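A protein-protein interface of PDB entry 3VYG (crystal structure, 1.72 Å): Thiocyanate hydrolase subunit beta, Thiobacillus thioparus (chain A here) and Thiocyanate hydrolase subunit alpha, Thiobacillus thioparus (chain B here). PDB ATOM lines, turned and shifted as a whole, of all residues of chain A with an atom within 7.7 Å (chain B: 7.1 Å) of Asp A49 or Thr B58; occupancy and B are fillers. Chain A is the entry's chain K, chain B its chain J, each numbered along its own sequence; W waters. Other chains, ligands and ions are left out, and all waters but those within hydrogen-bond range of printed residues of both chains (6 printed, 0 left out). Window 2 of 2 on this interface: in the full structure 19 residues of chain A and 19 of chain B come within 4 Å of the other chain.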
ATOM      1  N   ARG A  41      -1.049  17.973  30.221  1.00  0.00           N
ATOM      2  CA  ARG A  41      -0.561  18.755  29.078  1.00  0.00           C
ATOM      3  C   ARG A  41       0.904  18.575  28.848  1.00  0.00           C
ATOM      4  O   ARG A  41       1.355  18.350  27.663  1.00  0.00           O
ATOM      5  CB  ARG A  41      -1.007  20.215  29.241  1.00  0.00           C
ATOM      6  CG  ARG A  41      -0.683  21.025  27.920  1.00  0.00           C
ATOM      7  CD  ARG A  41      -0.958  22.519  28.128  1.00  0.00           C
ATOM      8  NE  ARG A  41      -0.645  23.211  26.849  1.00  0.00           N
ATOM      9  CZ  ARG A  41      -1.389  24.186  26.306  1.00  0.00           C
ATOM     10  NH1 ARG A  41      -2.516  24.568  26.907  1.00  0.00           N
ATOM     11  NH2 ARG A  41      -1.008  24.650  25.053  1.00  0.00           N
ATOM     12  N   ARG A  45       2.714  16.432  25.542  1.00  0.00           N
ATOM     13  CA  ARG A  45       3.248  17.503  24.618  1.00  0.00           C
ATOM     14  C   ARG A  45       3.922  16.806  23.474  1.00  0.00           C
ATOM     15  O   ARG A  45       4.340  15.639  23.620  1.00  0.00           O
ATOM     16  CB  ARG A  45       4.343  18.341  25.348  1.00  0.00           C
ATOM     17  CG  ARG A  45       5.514  17.362  25.596  1.00  0.00           C
ATOM     18  CD  ARG A  45       6.931  17.782  25.960  1.00  0.00           C
ATOM     19  NE  ARG A  45       7.293  18.978  25.318  1.00  0.00           N
ATOM     20  CZ  ARG A  45       8.502  19.500  25.314  1.00  0.00           C
ATOM     21  NH1 ARG A  45       9.555  18.917  25.899  1.00  0.00           N
ATOM     22  NH2 ARG A  45       8.613  20.683  24.798  1.00  0.00           N
ATOM     23  N   VAL A  46       4.092  17.440  22.317  1.00  0.00           N
ATOM     24  CA  VAL A  46       5.020  16.821  21.345  1.00  0.00           C
ATOM     25  C   VAL A  46       6.447  17.314  21.600  1.00  0.00           C
ATOM     26  O   VAL A  46       6.680  18.549  21.673  1.00  0.00           O
ATOM     27  CB  VAL A  46       4.625  17.212  19.900  1.00  0.00           C
ATOM     28  CG1 VAL A  46       3.678  16.115  19.399  1.00  0.00           C
ATOM     29  CG2 VAL A  46       3.967  18.536  19.927  1.00  0.00           C
ATOM     30  N   PRO A  47       7.414  16.409  21.673  1.00  0.00           N
ATOM     31  CA  PRO A  47       8.649  16.922  22.229  1.00  0.00           C
ATOM     32  C   PRO A  47       9.476  17.823  21.347  1.00  0.00           C
ATOM     33  O   PRO A  47      10.423  18.434  21.799  1.00  0.00           O
ATOM     34  CB  PRO A  47       9.487  15.674  22.518  1.00  0.00           C
ATOM     35  CG  PRO A  47       8.750  14.550  21.878  1.00  0.00           C
ATOM     36  CD  PRO A  47       7.315  14.916  21.744  1.00  0.00           C
ATOM     37  N   HIS A  48       9.120  17.896  20.048  1.00  0.00           N
ATOM     38  CA  HIS A  48       9.879  18.793  19.189  1.00  0.00           C
ATOM     39  C   HIS A  48       9.679  20.272  19.501  1.00  0.00           C
ATOM     40  O   HIS A  48      10.419  21.135  19.000  1.00  0.00           O
ATOM     41  CB  HIS A  48       9.564  18.488  17.679  1.00  0.00           C
ATOM     42  CG  HIS A  48       8.154  18.883  17.207  1.00  0.00           C
ATOM     43  ND1 HIS A  48       7.808  18.797  15.868  1.00  0.00           N
ATOM     44  CD2 HIS A  48       7.029  19.251  17.855  1.00  0.00           C
ATOM     45  CE1 HIS A  48       6.533  19.163  15.689  1.00  0.00           C
ATOM     46  NE2 HIS A  48       6.028  19.468  16.882  1.00  0.00           N
ATOM     47  N   ASP A  49       8.684  20.563  20.323  1.00  0.00           N
ATOM     48  CA  ASP A  49       8.253  21.963  20.543  1.00  0.00           C
ATOM     49  C   ASP A  49       9.022  22.636  21.672  1.00  0.00           C
ATOM     50  O   ASP A  49       8.477  22.771  22.783  1.00  0.00           O
ATOM     51  CB  ASP A  49       6.719  22.022  20.771  1.00  0.00           C
ATOM     52  CG  ASP A  49       6.166  23.408  20.784  1.00  0.00           C
ATOM     53  OD1 ASP A  49       6.832  24.399  20.501  1.00  0.00           O
ATOM     54  OD2 ASP A  49       4.984  23.487  21.147  1.00  0.00           O
ATOM     55  N   VAL A  50      10.251  23.045  21.346  1.00  0.00           N
ATOM     56  CA  VAL A  50      11.244  23.426  22.470  1.00  0.00           C
ATOM     57  C   VAL A  50      11.376  24.863  22.602  1.00  0.00           C
ATOM     58  O   VAL A  50      12.153  25.360  23.441  1.00  0.00           O
ATOM     59  CB  VAL A  50      12.641  22.727  22.295  1.00  0.00           C
ATOM     60  CG1 VAL A  50      12.451  21.179  22.364  1.00  0.00           C
ATOM     61  CG2 VAL A  50      13.427  23.187  21.007  1.00  0.00           C
ATOM     62  N   GLY A  51      10.787  25.619  21.639  1.00  0.00           N
ATOM     63  CA  GLY A  51      11.083  27.067  21.596  1.00  0.00           C
ATOM     64  C   GLY A  51      10.637  27.794  22.896  1.00  0.00           C
ATOM     65  O   GLY A  51       9.549  27.605  23.414  1.00  0.00           O
ATOM     66  N   GLY A  52      11.564  28.574  23.429  1.00  0.00           N
ATOM     67  CA  GLY A  52      11.298  29.350  24.674  1.00  0.00           C
ATOM     68  C   GLY A  52      11.732  28.624  25.988  1.00  0.00           C
ATOM     69  O   GLY A  52      11.675  29.210  27.050  1.00  0.00           O
ATOM     70  N   GLU A  53      12.059  27.349  25.890  1.00  0.00           N
ATOM     71  CA  GLU A  53      12.642  26.614  27.050  1.00  0.00           C
ATOM     72  C   GLU A  53      13.973  27.214  27.419  1.00  0.00           C
ATOM     73  O   GLU A  53      14.849  27.489  26.600  1.00  0.00           O
ATOM     74  CB  GLU A  53      12.855  25.167  26.603  1.00  0.00           C
ATOM     75  CG  GLU A  53      11.479  24.458  26.523  1.00  0.00           C
ATOM     76  CD  GLU A  53      11.612  23.017  26.172  1.00  0.00           C
ATOM     77  OE1 GLU A  53      12.709  22.495  26.267  1.00  0.00           O
ATOM     78  OE2 GLU A  53      10.631  22.397  25.792  1.00  0.00           O
ATOM     79  N   ASN A  95      10.258  13.157  15.151  1.00  0.00           N
ATOM     80  CA  ASN A  95      10.544  14.250  16.108  1.00  0.00           C
ATOM     81  C   ASN A  95       9.528  14.270  17.202  1.00  0.00           C
ATOM     82  O   ASN A  95       9.672  15.033  18.188  1.00  0.00           O
ATOM     83  CB  ASN A  95      10.553  15.631  15.370  1.00  0.00           C
ATOM     84  CG  ASN A  95      11.559  15.644  14.243  1.00  0.00           C
ATOM     85  OD1 ASN A  95      12.615  15.008  14.313  1.00  0.00           O
ATOM     86  ND2 ASN A  95      11.303  16.423  13.198  1.00  0.00           N
ATOM     87  N   CYS A  96       8.473  13.471  17.040  1.00  0.00           N
ATOM     88  CA  CYS A  96       7.401  13.461  18.055  1.00  0.00           C
ATOM     89  C   CYS A  96       7.064  12.081  18.608  1.00  0.00           C
ATOM     90  O   CYS A  96       7.136  11.845  19.857  1.00  0.00           O
ATOM     91  CB  CYS A  96       6.098  14.053  17.503  1.00  0.00           C
ATOM     92  SG  CYS A  96       6.357  15.817  16.945  1.00  0.00           S
ATOM     93  N   TYR A 103      14.010  11.346  22.221  1.00  0.00           N
ATOM     94  CA  TYR A 103      14.092  12.633  21.495  1.00  0.00           C
ATOM     95  C   TYR A 103      15.382  13.423  21.875  1.00  0.00           C
ATOM     96  O   TYR A 103      16.103  13.951  21.013  1.00  0.00           O
ATOM     97  CB  TYR A 103      12.806  13.462  21.691  1.00  0.00           C
ATOM     98  CG  TYR A 103      12.885  14.728  20.870  1.00  0.00           C
ATOM     99  CD1 TYR A 103      12.849  14.652  19.454  1.00  0.00           C
ATOM    100  CD2 TYR A 103      13.110  15.945  21.493  1.00  0.00           C
ATOM    101  CE1 TYR A 103      12.970  15.806  18.678  1.00  0.00           C
ATOM    102  CE2 TYR A 103      13.283  17.104  20.721  1.00  0.00           C
ATOM    103  CZ  TYR A 103      13.175  17.017  19.301  1.00  0.00           C
ATOM    104  OH  TYR A 103      13.370  18.148  18.527  1.00  0.00           O
ATOM    105  N   ASP B  47      -5.853  28.233  21.315  1.00  0.00           N
ATOM    106  CA  ASP B  47      -5.097  27.130  21.886  1.00  0.00           C
ATOM    107  C   ASP B  47      -5.800  25.829  21.642  1.00  0.00           C
ATOM    108  O   ASP B  47      -6.537  25.306  22.536  1.00  0.00           O
ATOM    109  CB  ASP B  47      -4.966  27.407  23.401  1.00  0.00           C
ATOM    110  CG  ASP B  47      -3.968  26.470  24.079  1.00  0.00           C
ATOM    111  OD1 ASP B  47      -3.191  25.772  23.349  1.00  0.00           O
ATOM    112  OD2 ASP B  47      -4.049  26.402  25.340  1.00  0.00           O
ATOM    113  N   ASP B  50      -3.599  19.751  21.227  1.00  0.00           N
ATOM    114  CA  ASP B  50      -2.389  19.489  20.534  1.00  0.00           C
ATOM    115  C   ASP B  50      -1.995  17.997  20.695  1.00  0.00           C
ATOM    116  O   ASP B  50      -0.846  17.581  20.380  1.00  0.00           O
ATOM    117  CB  ASP B  50      -1.258  20.454  21.034  1.00  0.00           C
ATOM    118  CG  ASP B  50      -0.856  20.174  22.523  1.00  0.00           C
ATOM    119  OD1 ASP B  50       0.286  20.545  22.971  1.00  0.00           O
ATOM    120  OD2 ASP B  50      -1.647  19.503  23.225  1.00  0.00           O
ATOM    121  N   THR B  54       1.304  18.778  16.359  1.00  0.00           N
ATOM    122  CA  THR B  54       0.941  20.143  15.961  1.00  0.00           C
ATOM    123  C   THR B  54       2.210  20.800  15.466  1.00  0.00           C
ATOM    124  O   THR B  54       3.329  20.444  15.915  1.00  0.00           O
ATOM    125  CB  THR B  54       0.336  21.024  17.114  1.00  0.00           C
ATOM    126  OG1 THR B  54       0.090  22.319  16.561  1.00  0.00           O
ATOM    127  CG2 THR B  54       1.311  21.227  18.215  1.00  0.00           C
ATOM    128  N   ARG B  55       2.068  21.752  14.549  1.00  0.00           N
ATOM    129  CA  ARG B  55       3.268  22.614  14.233  1.00  0.00           C
ATOM    130  C   ARG B  55       2.986  24.066  14.602  1.00  0.00           C
ATOM    131  O   ARG B  55       3.670  24.994  14.126  1.00  0.00           O
ATOM    132  CB  ARG B  55       3.638  22.522  12.699  1.00  0.00           C
ATOM    133  CG  ARG B  55       4.122  21.074  12.400  1.00  0.00           C
ATOM    134  CD  ARG B  55       4.785  21.066  10.993  1.00  0.00           C
ATOM    135  NE  ARG B  55       6.137  21.614  10.978  1.00  0.00           N
ATOM    136  CZ  ARG B  55       7.225  20.997  11.471  1.00  0.00           C
ATOM    137  NH1 ARG B  55       7.119  19.722  12.030  1.00  0.00           N
ATOM    138  NH2 ARG B  55       8.383  21.661  11.389  1.00  0.00           N
ATOM    139  N   THR B  56       1.986  24.299  15.474  1.00  0.00           N
ATOM    140  CA  THR B  56       1.759  25.651  16.003  1.00  0.00           C
ATOM    141  C   THR B  56       2.290  25.693  17.451  1.00  0.00           C
ATOM    142  O   THR B  56       1.686  25.121  18.328  1.00  0.00           O
ATOM    143  CB  THR B  56       0.237  25.978  15.994  1.00  0.00           C
ATOM    144  OG1 THR B  56      -0.169  25.912  14.596  1.00  0.00           O
ATOM    145  CG2 THR B  56       0.029  27.392  16.428  1.00  0.00           C
ATOM    146  N   MET B  57       3.474  26.274  17.561  1.00  0.00           N
ATOM    147  CA  MET B  57       4.315  26.130  18.800  1.00  0.00           C
ATOM    148  C   MET B  57       3.514  26.610  19.995  1.00  0.00           C
ATOM    149  O   MET B  57       2.741  27.554  19.919  1.00  0.00           O
ATOM    150  CB  MET B  57       5.558  27.039  18.694  1.00  0.00           C
ATOM    151  CG  MET B  57       6.629  26.600  17.688  1.00  0.00           C
ATOM    152  SD  MET B  57       6.058  26.916  15.911  1.00  0.00           S
ATOM    153  CE  MET B  57       6.060  28.669  15.875  1.00  0.00           C
ATOM    154  N   THR B  58       3.695  25.909  21.102  1.00  0.00           N
ATOM    155  CA  THR B  58       3.007  26.358  22.377  1.00  0.00           C
ATOM    156  C   THR B  58       3.286  27.801  22.687  1.00  0.00           C
ATOM    157  O   THR B  58       2.438  28.500  23.210  1.00  0.00           O
ATOM    158  CB  THR B  58       3.505  25.422  23.499  1.00  0.00           C
ATOM    159  OG1 THR B  58       3.138  24.090  23.218  1.00  0.00           O
ATOM    160  CG2 THR B  58       2.771  25.826  24.792  1.00  0.00           C
ATOM    161  N   TYR B  59       4.550  28.245  22.453  1.00  0.00           N
ATOM    162  CA  TYR B  59       4.891  29.624  22.789  1.00  0.00           C
ATOM    163  C   TYR B  59       3.993  30.684  22.120  1.00  0.00           C
ATOM    164  O   TYR B  59       4.011  31.792  22.548  1.00  0.00           O
ATOM    165  CB  TYR B  59       6.445  29.895  22.639  1.00  0.00           C
ATOM    166  CG  TYR B  59       6.953  30.075  21.207  1.00  0.00           C
ATOM    167  CD1 TYR B  59       6.696  31.251  20.530  1.00  0.00           C
ATOM    168  CD2 TYR B  59       7.735  29.155  20.645  1.00  0.00           C
ATOM    169  CE1 TYR B  59       7.114  31.462  19.212  1.00  0.00           C
ATOM    170  CE2 TYR B  59       8.243  29.335  19.272  1.00  0.00           C
ATOM    171  CZ  TYR B  59       7.904  30.557  18.627  1.00  0.00           C
ATOM    172  OH  TYR B  59       8.442  30.732  17.342  1.00  0.00           O
ATOM    173  N   THR B  60       3.313  30.307  21.036  1.00  0.00           N
ATOM    174  CA  THR B  60       2.400  31.277  20.347  1.00  0.00           C
ATOM    175  C   THR B  60       0.943  31.275  20.939  1.00  0.00           C
ATOM    176  O   THR B  60       0.213  32.160  20.593  1.00  0.00           O
ATOM    177  CB  THR B  60       2.272  31.040  18.830  1.00  0.00           C
ATOM    178  OG1 THR B  60       1.557  29.804  18.582  1.00  0.00           O
ATOM    179  CG2 THR B  60       3.627  31.024  18.183  1.00  0.00           C
ATOM    180  N   ARG B  61       0.517  30.287  21.761  1.00  0.00           N
ATOM    181  CA  ARG B  61      -0.894  30.081  22.003  1.00  0.00           C
ATOM    182  C   ARG B  61      -1.415  31.273  22.870  1.00  0.00           C
ATOM    183  O   ARG B  61      -0.775  31.724  23.851  1.00  0.00           O
ATOM    184  CB  ARG B  61      -1.166  28.728  22.763  1.00  0.00           C
ATOM    185  CG  ARG B  61      -0.576  27.471  22.034  1.00  0.00           C
ATOM    186  CD  ARG B  61      -0.987  27.447  20.602  1.00  0.00           C
ATOM    187  NE  ARG B  61      -0.536  26.208  19.965  1.00  0.00           N
ATOM    188  CZ  ARG B  61      -1.315  25.110  19.914  1.00  0.00           C
ATOM    189  NH1 ARG B  61      -2.466  25.056  20.567  1.00  0.00           N
ATOM    190  NH2 ARG B  61      -0.937  24.054  19.235  1.00  0.00           N
ATOM    191  N   GLY B  62      -2.486  31.862  22.353  1.00  0.00           N
ATOM    192  CA  GLY B  62      -3.143  32.958  23.082  1.00  0.00           C
ATOM    193  C   GLY B  62      -2.514  34.310  22.808  1.00  0.00           C
ATOM    194  O   GLY B  62      -2.992  35.323  23.352  1.00  0.00           O
ATOM    195  N   TRP B 102       7.110  36.948  25.612  1.00  0.00           N
ATOM    196  CA  TRP B 102       7.973  36.629  26.767  1.00  0.00           C
ATOM    197  C   TRP B 102       7.828  37.782  27.761  1.00  0.00           C
ATOM    198  O   TRP B 102       8.191  38.925  27.467  1.00  0.00           O
ATOM    199  CB  TRP B 102       9.452  36.581  26.307  1.00  0.00           C
ATOM    200  CG  TRP B 102       9.607  35.803  25.003  1.00  0.00           C
ATOM    201  CD1 TRP B 102       9.987  36.346  23.782  1.00  0.00           C
ATOM    202  CD2 TRP B 102       9.318  34.415  24.769  1.00  0.00           C
ATOM    203  NE1 TRP B 102      10.026  35.345  22.811  1.00  0.00           N
ATOM    204  CE2 TRP B 102       9.653  34.151  23.372  1.00  0.00           C
ATOM    205  CE3 TRP B 102       8.830  33.372  25.562  1.00  0.00           C
ATOM    206  CZ2 TRP B 102       9.435  32.895  22.760  1.00  0.00           C
ATOM    207  CZ3 TRP B 102       8.654  32.083  24.957  1.00  0.00           C
ATOM    208  CH2 TRP B 102       8.978  31.879  23.574  1.00  0.00           C
HETATM  209  O   HOH W   1       1.312  22.528  24.996  1.00  0.00           O
HETATM  210  O   HOH W   2       0.196  23.631  22.544  1.00  0.00           O
HETATM  211  O   HOH W   3       9.394  18.603  13.510  1.00  0.00           O
HETATM  212  O   HOH W   4      -2.765  21.304  25.013  1.00  0.00           O
HETATM  213  O   HOH W   5       6.737  26.293  22.372  1.00  0.00           O
HETATM  214  O   HOH W   6      -3.489  23.073  23.463  1.00  0.00           O
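Of the 12 printed residues of chain B, 7 touch a printed residue of chain A.
Printed residues of chain B that touch a printed residue of chain A: Asp B47, Thr B54, Arg B55, Met B57, Thr B58, Tyr B59 and Trp B102.
Hydrophobic or aromatic side chains of chain B that line the printed part of chain A: Met B57, Tyr B59 and Trp B102.
Of the 13 printed residues of chain A, 5 touch a printed residue of chain B.
Printed residues of chain A that touch a printed residue of chain B: Arg A41, His A48, Asp A49, Gly A51 and Gly A52.
Hydrophobic or aromatic side chains of chain A within 4 Å of the printed part of chain B: His A48.
Among the printed residues, 8 pairs touch across the chains.
The backbone carbonyl oxygen (O) of Thr B54 sits at hydrogen-bond distance from a ring nitrogen (NE2) of His A48.
N of Thr B58 is in hydrogen-bond range of OD2 of Asp A49, 2.7 Å away.
The guanidinium group of Arg A41 lies within salt-bridge range of the side-chain carboxylate of Asp B47 (2.9 Å).
Among the printed residues, pairs that only touch across the chains: Asp A49 with Met B57 (3.4 Å), Gly A52 with Trp B102 (3.6 Å), Gly A51 with Tyr B59 (3.7 Å), His A48 with Arg B55 (3.7 Å) and Arg A41 with Thr B58 (3.97 Å).
Of chain B, only Met B57 (3.4 Å) and Thr B58 (2.7 Å) come within 4 Å of Asp A49.
Of the printed residues of chain A, Thr B54 touches His A48.
Printed residues of chain B within 4 Å of His A48: Thr B54 (3.0 Å) and Arg B55 (3.7 Å).
Of the printed residues of chain A, Arg B55 touches His A48 (3.7 Å).
Of the printed residues of chain A, Met B57 touches Asp A49 (3.4 Å).
Printed residues of chain B within 4 Å of Arg A41: Asp B47 (2.9 Å) and Thr B58 (3.97 Å).
Arg A45 touches none of the printed residues of chain B.
Val A50 touches none of the printed residues of chain B.
The nearest residue of chain B that does not touch Asp A49 is Thr B56 (4.6 Å).
The nearest printed residue of chain A that does not touch Asp B47 is Asp A49 (8.8 Å).
Water W5 lies within hydrogen-bond range of the side-chain carboxylate (OD1) of Asp A49, the backbone NH (N) of Tyr B59, the backbone carbonyl oxygen (O) of Gly A51 and the backbone NH (N) of Thr B58.
Water W6 lies within hydrogen-bond range of OD1 of Asp B47 (2.7 Å) and NH2 of Arg A41 (3.3 Å).
Water W4 lies within hydrogen-bond range of the side-chain carboxylate (OD2) of Asp B50 and the guanidinium group (NE) of Arg A41.
Water W1 lies within hydrogen-bond range of NE of Arg A41 (2.8 Å), OG1 of Thr B58 (3.0 Å) and OD1 of Asp B50 (3.0 Å).
Water W3 lies within hydrogen-bond range of a ring nitrogen (ND1) of His A48, the side-chain amide nitrogen of Asn A95 and the guanidinium group of Arg B55.
Water W2 lies within hydrogen-bond range of NH2 of Arg A41 (3.0 Å), OG1 of Thr B58 (3.1 Å) and OD1 of Asp B50 (3.1 Å).
A ring nitrogen (ND1) of His A48 sits at hydrogen-bond distance from the side-chain sulfur of Cys A96.
NH2 of Arg B61 is in hydrogen-bond range of OG1 of Thr B54, 3.3 Å away.
The backbone NH (N) of Thr B56 lies within hydrogen-bond range of the side-chain hydroxyl (OG1) of Thr B54, 2.9 Å away.
The backbone carbonyl oxygen of Met B57 is in hydrogen-bond range of the side-chain hydroxyl of Thr B60, at 2.9 Å.
The backbone NH (N) of His A48 is in hydrogen-bond range of the backbone carbonyl oxygen (O) of Asn A95 (3.5 Å).
NH2 of Arg A45 sits at hydrogen-bond distance from O of Asp A49, 2.9 Å away.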
